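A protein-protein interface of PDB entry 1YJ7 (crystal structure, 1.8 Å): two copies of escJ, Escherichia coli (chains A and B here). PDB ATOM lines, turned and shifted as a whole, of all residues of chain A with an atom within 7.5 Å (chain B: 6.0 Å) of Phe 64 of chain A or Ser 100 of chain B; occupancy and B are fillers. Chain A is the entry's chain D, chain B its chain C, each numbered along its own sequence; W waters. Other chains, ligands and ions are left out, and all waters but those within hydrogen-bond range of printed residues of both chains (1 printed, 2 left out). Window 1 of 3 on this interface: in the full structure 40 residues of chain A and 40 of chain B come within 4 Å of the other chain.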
ATOM      1  N   ASN A  57      -8.115 -14.961  -6.077  1.00  0.00           N
ATOM      2  CA  ASN A  57      -8.481 -15.240  -4.691  1.00  0.00           C
ATOM      3  C   ASN A  57      -9.655 -16.193  -4.535  1.00  0.00           C
ATOM      4  O   ASN A  57     -10.149 -16.397  -3.422  1.00  0.00           O
ATOM      5  CB  ASN A  57      -8.740 -13.921  -3.960  1.00  0.00           C
ATOM      6  CG  ASN A  57      -7.468 -13.194  -3.646  1.00  0.00           C
ATOM      7  OD1 ASN A  57      -6.819 -13.492  -2.637  1.00  0.00           O
ATOM      8  ND2 ASN A  57      -7.047 -12.293  -4.533  1.00  0.00           N
ATOM      9  N   GLY A  58     -10.100 -16.761  -5.652  1.00  0.00           N
ATOM     10  CA  GLY A  58     -11.106 -17.796  -5.664  1.00  0.00           C
ATOM     11  C   GLY A  58     -12.518 -17.331  -5.434  1.00  0.00           C
ATOM     12  O   GLY A  58     -13.336 -18.118  -4.933  1.00  0.00           O
ATOM     13  N   LYS A  61     -16.939 -17.942  -4.396  1.00  0.00           N
ATOM     14  CA  LYS A  61     -16.611 -19.285  -3.947  1.00  0.00           C
ATOM     15  C   LYS A  61     -17.551 -20.283  -4.580  1.00  0.00           C
ATOM     16  O   LYS A  61     -18.750 -20.066  -4.653  1.00  0.00           O
ATOM     17  CB  LYS A  61     -16.684 -19.387  -2.426  1.00  0.00           C
ATOM     18  CG  LYS A  61     -15.736 -18.462  -1.695  1.00  0.00           C
ATOM     19  CD  LYS A  61     -14.324 -18.981  -1.692  1.00  0.00           C
ATOM     20  CE  LYS A  61     -13.399 -18.045  -0.937  1.00  0.00           C
ATOM     21  NZ  LYS A  61     -12.058 -18.001  -1.573  1.00  0.00           N
ATOM     22  N   LYS A  62     -16.995 -21.372  -5.086  1.00  0.00           N
ATOM     23  CA  LYS A  62     -17.838 -22.354  -5.731  1.00  0.00           C
ATOM     24  C   LYS A  62     -18.495 -23.248  -4.696  1.00  0.00           C
ATOM     25  O   LYS A  62     -18.006 -23.383  -3.571  1.00  0.00           O
ATOM     26  CB  LYS A  62     -17.104 -23.109  -6.850  1.00  0.00           C
ATOM     27  CG  LYS A  62     -15.996 -24.017  -6.462  1.00  0.00           C
ATOM     28  CD  LYS A  62     -15.359 -24.628  -7.720  1.00  0.00           C
ATOM     29  CE  LYS A  62     -16.221 -25.720  -8.338  1.00  0.00           C
ATOM     30  NZ  LYS A  62     -15.536 -26.422  -9.475  1.00  0.00           N
ATOM     31  N   LYS A  63     -19.655 -23.769  -5.073  1.00  0.00           N
ATOM     32  CA  LYS A  63     -20.413 -24.713  -4.275  1.00  0.00           C
ATOM     33  C   LYS A  63     -20.048 -26.141  -4.691  1.00  0.00           C
ATOM     34  O   LYS A  63     -19.624 -26.389  -5.821  1.00  0.00           O
ATOM     35  CB  LYS A  63     -21.912 -24.487  -4.472  1.00  0.00           C
ATOM     36  CG  LYS A  63     -22.430 -23.114  -4.007  1.00  0.00           C
ATOM     37  CD  LYS A  63     -22.493 -22.998  -2.482  1.00  0.00           C
ATOM     38  CE  LYS A  63     -23.589 -23.892  -1.878  1.00  0.00           C
ATOM     39  NZ  LYS A  63     -24.037 -23.440  -0.519  1.00  0.00           N
ATOM     40  N   PHE A  64     -20.193 -27.071  -3.760  1.00  0.00           N
ATOM     41  CA  PHE A  64     -19.977 -28.484  -4.041  1.00  0.00           C
ATOM     42  C   PHE A  64     -21.222 -29.289  -3.672  1.00  0.00           C
ATOM     43  O   PHE A  64     -22.131 -28.769  -3.034  1.00  0.00           O
ATOM     44  CB  PHE A  64     -18.741 -28.979  -3.294  1.00  0.00           C
ATOM     45  CG  PHE A  64     -17.530 -28.174  -3.584  1.00  0.00           C
ATOM     46  CD1 PHE A  64     -17.265 -27.034  -2.855  1.00  0.00           C
ATOM     47  CD2 PHE A  64     -16.680 -28.516  -4.627  1.00  0.00           C
ATOM     48  CE1 PHE A  64     -16.141 -26.254  -3.139  1.00  0.00           C
ATOM     49  CE2 PHE A  64     -15.549 -27.731  -4.911  1.00  0.00           C
ATOM     50  CZ  PHE A  64     -15.295 -26.618  -4.161  1.00  0.00           C
ATOM     51  N   ALA A  65     -21.252 -30.556  -4.066  1.00  0.00           N
ATOM     52  CA  ALA A  65     -22.449 -31.384  -3.873  1.00  0.00           C
ATOM     53  C   ALA A  65     -22.831 -31.481  -2.406  1.00  0.00           C
ATOM     54  O   ALA A  65     -21.978 -31.625  -1.521  1.00  0.00           O
ATOM     55  CB  ALA A  65     -22.248 -32.768  -4.450  1.00  0.00           C
ATOM     56  N   ASP A  66     -24.134 -31.392  -2.170  1.00  0.00           N
ATOM     57  CA  ASP A  66     -24.714 -31.471  -0.851  1.00  0.00           C
ATOM     58  C   ASP A  66     -25.216 -32.905  -0.692  1.00  0.00           C
ATOM     59  O   ASP A  66     -25.956 -33.397  -1.527  1.00  0.00           O
ATOM     60  CB  ASP A  66     -25.868 -30.465  -0.767  1.00  0.00           C
ATOM     61  CG  ASP A  66     -26.545 -30.430   0.595  1.00  0.00           C
ATOM     62  OD1 ASP A  66     -27.405 -29.534   0.777  1.00  0.00           O
ATOM     63  OD2 ASP A  66     -26.320 -31.231   1.526  1.00  0.00           O
ATOM     64  N   ILE A  67     -24.804 -33.579   0.373  1.00  0.00           N
ATOM     65  CA  ILE A  67     -25.250 -34.953   0.619  1.00  0.00           C
ATOM     66  C   ILE A  67     -26.780 -35.060   0.687  1.00  0.00           C
ATOM     67  O   ILE A  67     -27.343 -36.066   0.289  1.00  0.00           O
ATOM     68  CB  ILE A  67     -24.605 -35.512   1.910  1.00  0.00           C
ATOM     69  CG1 ILE A  67     -24.911 -36.998   2.074  1.00  0.00           C
ATOM     70  CG2 ILE A  67     -25.015 -34.703   3.147  1.00  0.00           C
ATOM     71  CD1 ILE A  67     -24.030 -37.659   3.137  1.00  0.00           C
ATOM     72  N   VAL A  69     -28.893 -33.406  -1.039  1.00  0.00           N
ATOM     73  CA  VAL A  69     -29.415 -33.353  -2.404  1.00  0.00           C
ATOM     74  C   VAL A  69     -29.159 -34.665  -3.142  1.00  0.00           C
ATOM     75  O   VAL A  69     -30.067 -35.195  -3.779  1.00  0.00           O
ATOM     76  CB  VAL A  69     -28.800 -32.177  -3.191  1.00  0.00           C
ATOM     77  CG1 VAL A  69     -29.261 -32.197  -4.656  1.00  0.00           C
ATOM     78  CG2 VAL A  69     -29.159 -30.859  -2.526  1.00  0.00           C
ATOM     79  N   ASP A 107     -11.394 -21.960   9.912  1.00  0.00           N
ATOM     80  CA  ASP A 107     -12.089 -22.852   8.986  1.00  0.00           C
ATOM     81  C   ASP A 107     -11.481 -24.248   9.171  1.00  0.00           C
ATOM     82  O   ASP A 107     -10.362 -24.358   9.647  1.00  0.00           O
ATOM     83  CB  ASP A 107     -11.965 -22.359   7.537  1.00  0.00           C
ATOM     84  CG  ASP A 107     -13.029 -22.920   6.614  1.00  0.00           C
ATOM     85  OD1 ASP A 107     -13.071 -22.471   5.438  1.00  0.00           O
ATOM     86  OD2 ASP A 107     -13.853 -23.805   6.921  1.00  0.00           O
ATOM     87  N   SER A 109     -11.873 -28.538   7.534  1.00  0.00           N
ATOM     88  CA  SER A 109     -12.499 -29.598   6.783  1.00  0.00           C
ATOM     89  C   SER A 109     -11.966 -30.929   7.258  1.00  0.00           C
ATOM     90  O   SER A 109     -10.775 -31.074   7.468  1.00  0.00           O
ATOM     91  CB  SER A 109     -12.231 -29.468   5.282  1.00  0.00           C
ATOM     92  OG  SER A 109     -13.019 -28.455   4.699  1.00  0.00           O
ATOM     93  N   LEU A 127      -7.937 -30.593   7.400  1.00  0.00           N
ATOM     94  CA  LEU A 127      -7.366 -29.310   6.991  1.00  0.00           C
ATOM     95  C   LEU A 127      -7.889 -28.238   7.939  1.00  0.00           C
ATOM     96  O   LEU A 127      -9.108 -28.120   8.168  1.00  0.00           O
ATOM     97  CB  LEU A 127      -7.768 -28.971   5.568  1.00  0.00           C
ATOM     98  CG  LEU A 127      -7.309 -27.605   5.044  1.00  0.00           C
ATOM     99  CD1 LEU A 127      -5.798 -27.498   4.977  1.00  0.00           C
ATOM    100  CD2 LEU A 127      -7.941 -27.352   3.699  1.00  0.00           C
ATOM    101  N   GLN B  93     -16.499 -34.902  -4.409  1.00  0.00           N
ATOM    102  CA  GLN B  93     -16.946 -33.556  -4.064  1.00  0.00           C
ATOM    103  C   GLN B  93     -16.445 -33.112  -2.676  1.00  0.00           C
ATOM    104  O   GLN B  93     -16.051 -31.971  -2.496  1.00  0.00           O
ATOM    105  CB  GLN B  93     -18.458 -33.480  -4.167  1.00  0.00           C
ATOM    106  CG  GLN B  93     -18.959 -33.624  -5.613  1.00  0.00           C
ATOM    107  CD  GLN B  93     -18.662 -32.414  -6.460  1.00  0.00           C
ATOM    108  OE1 GLN B  93     -17.932 -32.499  -7.473  1.00  0.00           O
ATOM    109  NE2 GLN B  93     -19.215 -31.294  -6.072  1.00  0.00           N
ATOM    110  N   ASP B  94     -16.450 -34.026  -1.711  1.00  0.00           N
ATOM    111  CA  ASP B  94     -15.922 -33.732  -0.376  1.00  0.00           C
ATOM    112  C   ASP B  94     -14.442 -33.376  -0.452  1.00  0.00           C
ATOM    113  O   ASP B  94     -13.985 -32.453   0.231  1.00  0.00           O
ATOM    114  CB  ASP B  94     -16.078 -34.922   0.567  1.00  0.00           C
ATOM    115  CG  ASP B  94     -17.513 -35.205   0.971  1.00  0.00           C
ATOM    116  OD1 ASP B  94     -18.447 -34.360   0.775  1.00  0.00           O
ATOM    117  OD2 ASP B  94     -17.779 -36.300   1.541  1.00  0.00           O
ATOM    118  N   ILE B  95     -13.680 -34.113  -1.257  1.00  0.00           N
ATOM    119  CA  ILE B  95     -12.252 -33.869  -1.377  1.00  0.00           C
ATOM    120  C   ILE B  95     -12.016 -32.546  -2.105  1.00  0.00           C
ATOM    121  O   ILE B  95     -11.167 -31.762  -1.695  1.00  0.00           O
ATOM    122  CB  ILE B  95     -11.517 -35.047  -2.079  1.00  0.00           C
ATOM    123  CG1 ILE B  95     -11.594 -36.304  -1.207  1.00  0.00           C
ATOM    124  CG2 ILE B  95     -10.085 -34.704  -2.289  1.00  0.00           C
ATOM    125  CD1 ILE B  95     -11.209 -37.559  -1.944  1.00  0.00           C
ATOM    126  N   GLU B  96     -12.783 -32.287  -3.160  1.00  0.00           N
ATOM    127  CA  GLU B  96     -12.670 -31.001  -3.859  1.00  0.00           C
ATOM    128  C   GLU B  96     -12.975 -29.851  -2.893  1.00  0.00           C
ATOM    129  O   GLU B  96     -12.293 -28.836  -2.913  1.00  0.00           O
ATOM    130  CB  GLU B  96     -13.568 -30.931  -5.085  1.00  0.00           C
ATOM    131  CG  GLU B  96     -13.131 -31.840  -6.224  1.00  0.00           C
ATOM    132  CD  GLU B  96     -14.072 -31.799  -7.423  1.00  0.00           C
ATOM    133  OE1 GLU B  96     -13.968 -32.686  -8.307  1.00  0.00           O
ATOM    134  OE2 GLU B  96     -14.934 -30.904  -7.461  1.00  0.00           O
ATOM    135  N   ARG B  97     -14.010 -30.003  -2.080  1.00  0.00           N
ATOM    136  CA  ARG B  97     -14.391 -28.962  -1.118  1.00  0.00           C
ATOM    137  C   ARG B  97     -13.250 -28.677  -0.143  1.00  0.00           C
ATOM    138  O   ARG B  97     -12.932 -27.514   0.148  1.00  0.00           O
ATOM    139  CB  ARG B  97     -15.659 -29.380  -0.371  1.00  0.00           C
ATOM    140  CG  ARG B  97     -16.131 -28.352   0.633  1.00  0.00           C
ATOM    141  CD  ARG B  97     -17.104 -28.870   1.606  1.00  0.00           C
ATOM    142  NE  ARG B  97     -18.412 -28.772   1.004  1.00  0.00           N
ATOM    143  CZ  ARG B  97     -19.124 -29.766   0.573  1.00  0.00           C
ATOM    144  NH1 ARG B  97     -18.679 -31.010   0.705  1.00  0.00           N
ATOM    145  NH2 ARG B  97     -20.317 -29.518   0.032  1.00  0.00           N
ATOM    146  N   LEU B  98     -12.626 -29.740   0.359  1.00  0.00           N
ATOM    147  CA  LEU B  98     -11.517 -29.609   1.312  1.00  0.00           C
ATOM    148  C   LEU B  98     -10.310 -28.945   0.632  1.00  0.00           C
ATOM    149  O   LEU B  98      -9.759 -27.966   1.143  1.00  0.00           O
ATOM    150  CB  LEU B  98     -11.146 -30.978   1.875  1.00  0.00           C
ATOM    151  CG  LEU B  98      -9.999 -31.068   2.908  1.00  0.00           C
ATOM    152  CD1 LEU B  98     -10.238 -32.276   3.824  1.00  0.00           C
ATOM    153  CD2 LEU B  98      -8.637 -31.126   2.266  1.00  0.00           C
ATOM    154  N   LEU B  99      -9.913 -29.443  -0.539  1.00  0.00           N
ATOM    155  CA  LEU B  99      -8.722 -28.895  -1.224  1.00  0.00           C
ATOM    156  C   LEU B  99      -8.925 -27.443  -1.638  1.00  0.00           C
ATOM    157  O   LEU B  99      -7.978 -26.655  -1.695  1.00  0.00           O
ATOM    158  CB  LEU B  99      -8.350 -29.724  -2.460  1.00  0.00           C
ATOM    159  CG  LEU B  99      -7.947 -31.175  -2.164  1.00  0.00           C
ATOM    160  CD1 LEU B  99      -7.669 -31.883  -3.489  1.00  0.00           C
ATOM    161  CD2 LEU B  99      -6.768 -31.246  -1.246  1.00  0.00           C
ATOM    162  N   SER B 100     -10.179 -27.079  -1.892  1.00  0.00           N
ATOM    163  CA  SER B 100     -10.499 -25.722  -2.314  1.00  0.00           C
ATOM    164  C   SER B 100     -10.362 -24.680  -1.197  1.00  0.00           C
ATOM    165  O   SER B 100     -10.392 -23.464  -1.468  1.00  0.00           O
ATOM    166  CB  SER B 100     -11.888 -25.672  -2.942  1.00  0.00           C
ATOM    167  OG  SER B 100     -11.912 -26.475  -4.109  1.00  0.00           O
ATOM    168  N   LYS B 101     -10.190 -25.132   0.048  1.00  0.00           N
ATOM    169  CA  LYS B 101      -9.861 -24.235   1.157  1.00  0.00           C
ATOM    170  C   LYS B 101      -8.364 -23.964   1.320  1.00  0.00           C
ATOM    171  O   LYS B 101      -7.966 -23.103   2.103  1.00  0.00           O
ATOM    172  CB  LYS B 101     -10.439 -24.771   2.466  1.00  0.00           C
ATOM    173  CG  LYS B 101     -11.923 -24.910   2.464  1.00  0.00           C
ATOM    174  CD  LYS B 101     -12.423 -25.332   3.838  1.00  0.00           C
ATOM    175  CE  LYS B 101     -13.897 -25.681   3.825  1.00  0.00           C
ATOM    176  NZ  LYS B 101     -14.343 -26.067   5.211  1.00  0.00           N
ATOM    177  N   ILE B 102      -7.517 -24.713   0.616  1.00  0.00           N
ATOM    178  CA  ILE B 102      -6.074 -24.455   0.666  1.00  0.00           C
ATOM    179  C   ILE B 102      -5.752 -23.129  -0.026  1.00  0.00           C
ATOM    180  O   ILE B 102      -6.117 -22.954  -1.189  1.00  0.00           O
ATOM    181  CB  ILE B 102      -5.292 -25.614  -0.003  1.00  0.00           C
ATOM    182  CG1 ILE B 102      -5.555 -26.921   0.744  1.00  0.00           C
ATOM    183  CG2 ILE B 102      -3.797 -25.276  -0.071  1.00  0.00           C
ATOM    184  CD1 ILE B 102      -4.938 -28.164   0.086  1.00  0.00           C
ATOM    185  N   PRO B 103      -5.092 -22.186   0.661  1.00  0.00           N
ATOM    186  CA  PRO B 103      -4.743 -20.909   0.035  1.00  0.00           C
ATOM    187  C   PRO B 103      -3.998 -21.087  -1.285  1.00  0.00           C
ATOM    188  O   PRO B 103      -3.031 -21.868  -1.356  1.00  0.00           O
ATOM    189  CB  PRO B 103      -3.851 -20.240   1.088  1.00  0.00           C
ATOM    190  CG  PRO B 103      -4.357 -20.790   2.370  1.00  0.00           C
ATOM    191  CD  PRO B 103      -4.654 -22.230   2.072  1.00  0.00           C
ATOM    192  N   VAL B 105      -5.523 -22.312  -4.094  1.00  0.00           N
ATOM    193  CA  VAL B 105      -6.320 -23.176  -4.966  1.00  0.00           C
ATOM    194  C   VAL B 105      -7.506 -22.387  -5.487  1.00  0.00           C
ATOM    195  O   VAL B 105      -8.259 -21.850  -4.687  1.00  0.00           O
ATOM    196  CB  VAL B 105      -6.828 -24.428  -4.221  1.00  0.00           C
ATOM    197  CG1 VAL B 105      -7.782 -25.248  -5.116  1.00  0.00           C
ATOM    198  CG2 VAL B 105      -5.656 -25.291  -3.753  1.00  0.00           C
ATOM    199  N   ASP B 107      -9.341 -23.739  -8.459  1.00  0.00           N
ATOM    200  CA  ASP B 107     -10.210 -24.763  -9.027  1.00  0.00           C
ATOM    201  C   ASP B 107      -9.562 -26.121  -8.776  1.00  0.00           C
ATOM    202  O   ASP B 107      -8.372 -26.206  -8.543  1.00  0.00           O
ATOM    203  CB  ASP B 107     -10.432 -24.528 -10.535  1.00  0.00           C
ATOM    204  CG  ASP B 107     -11.698 -25.192 -11.058  1.00  0.00           C
ATOM    205  OD1 ASP B 107     -12.016 -24.973 -12.257  1.00  0.00           O
ATOM    206  OD2 ASP B 107     -12.428 -25.936 -10.373  1.00  0.00           O
ATOM    207  N   CYS B 108     -10.365 -27.177  -8.784  1.00  0.00           N
ATOM    208  CA  CYS B 108      -9.914 -28.521  -8.411  1.00  0.00           C
ATOM    209  C   CYS B 108     -10.862 -29.525  -9.056  1.00  0.00           C
ATOM    210  O   CYS B 108     -12.071 -29.289  -9.106  1.00  0.00           O
ATOM    211  CB  CYS B 108      -9.988 -28.697  -6.865  1.00  0.00           C
ATOM    212  SG  CYS B 108      -9.386 -30.282  -6.301  1.00  0.00           S
HETATM  213  O   HOH W   1     -13.719 -27.605  -7.856  1.00  0.00           O
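NZ of Lys 62 of chain A lies within salt-bridge range of OD2 of Asp 107 of chain B, at 3.3 Å. The side-chain hydroxyl (OG) of Ser 109 of chain A lies within hydrogen-bond range of the side-chain amino group (NZ) of Lys 101 of chain B (2.8 Å). The backbone NH (N) of Ala 65 of chain A sits close to the side-chain amide nitrogen (NE2) of Gln 93 of chain B. NH2 of Arg 97 of chain B sits at hydrogen-bond distance from O of Ala 65 of chain A, 3.1 Å away. NZ of Lys 101 of chain B is in salt-bridge range of OD2 of Asp 107 of chain A, 2.9 Å away.
The guanidinium group of Arg 97 of chain B is in salt-bridge range of the side-chain carboxylate of Asp 94 of chain B, 3.4 Å away. The backbone carbonyl oxygen (O) of Glu 96 of chain B lies within hydrogen-bond range of the side-chain hydroxyl (OG) of Ser 100 of chain B, 2.7 Å away. The side-chain amide oxygen of Gln 93 of chain B lies close to the side-chain carboxylate of Glu 96 of chain B, 3.4 Å away. N of Ser 109 of chain A sits at hydrogen-bond distance from O of Leu 127 of chain A, at 2.9 Å.
Phe 64 of chain A touches Gln 93 of chain B. CB of Glu 96 of chain B touches CE2 of Phe 64 of chain A (3.8 Å). Phe 64 of chain A touches Arg 97 of chain B. Phe 64 of chain A touches Ser 100 of chain B (CZ to OG, 3.4 Å). Leu 98 of chain B touches Ser 109 of chain A. Leu 127 of chain A touches Leu 98 of chain B. Lys 101 of chain B touches Leu 127 of chain A. Ile 102 of chain B touches Leu 127 of chain A.
Printed residues of chain B within 4 Å of Lys 62 of chain A: Asp 107 (3.3 Å). Of chain B, only Gln 93 (3.5 Å), Glu 96 (3.8 Å), Arg 97 (3.6 Å) and Ser 100 (3.4 Å) come within 4 Å of Phe 64 of chain A. Printed residues of chain B within 4 Å of Asp 107 of chain A: Lys 101 (2.9 Å). Printed residues of chain A within 4 Å of Gln 93 of chain B: Phe 64 (3.5 Å) and Ala 65 (3.0 Å). Printed residues of chain A within 4 Å of Arg 97 of chain B: Phe 64 (3.6 Å) and Ala 65 (3.1 Å). Ser 100 of chain B touches one residue of chain A. Printed residues of chain A within 4 Å of Lys 101 of chain B: Asp 107 (2.9 Å), Ser 109 (2.8 Å) and Leu 127 (3.8 Å). Pro 103 of chain B touches none of the printed residues of chain A. The nearest residue of chain B that does not touch Phe 64 of chain A is Cys 108 of chain B (5.7 Å).
Of the 13 printed residues of chain A, 6 touch a printed residue of chain B. Hydrophobic or aromatic side chains of chain A that line the printed part of chain B: Phe 64, Ala 65 and Leu 127. Printed residues of chain B that touch a printed residue of chain A: Gln 93, Glu 96, Arg 97, Leu 98, Ser 100, Lys 101, Ile 102 and Asp 107. Hydrophobic or aromatic side chains of chain B within 4 Å of the printed part of chain A: Leu 98 and Ile 102. Among the printed residues, 13 pairs touch across the chains.
1 position is printed for both chains. Of the 13 pairs that touch across the chains among the printed residues, none has its exchanged pair printed and touching as well.
Water W1 lies within hydrogen-bond range of the backbone carbonyl oxygen (O) of Cys 108 of chain B (2.7 Å), the side-chain amino group (NZ) of Lys 62 of chain A (2.7 Å) and the side-chain carboxylate (OD2) of Asp 107 of chain B (3.3 Å).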
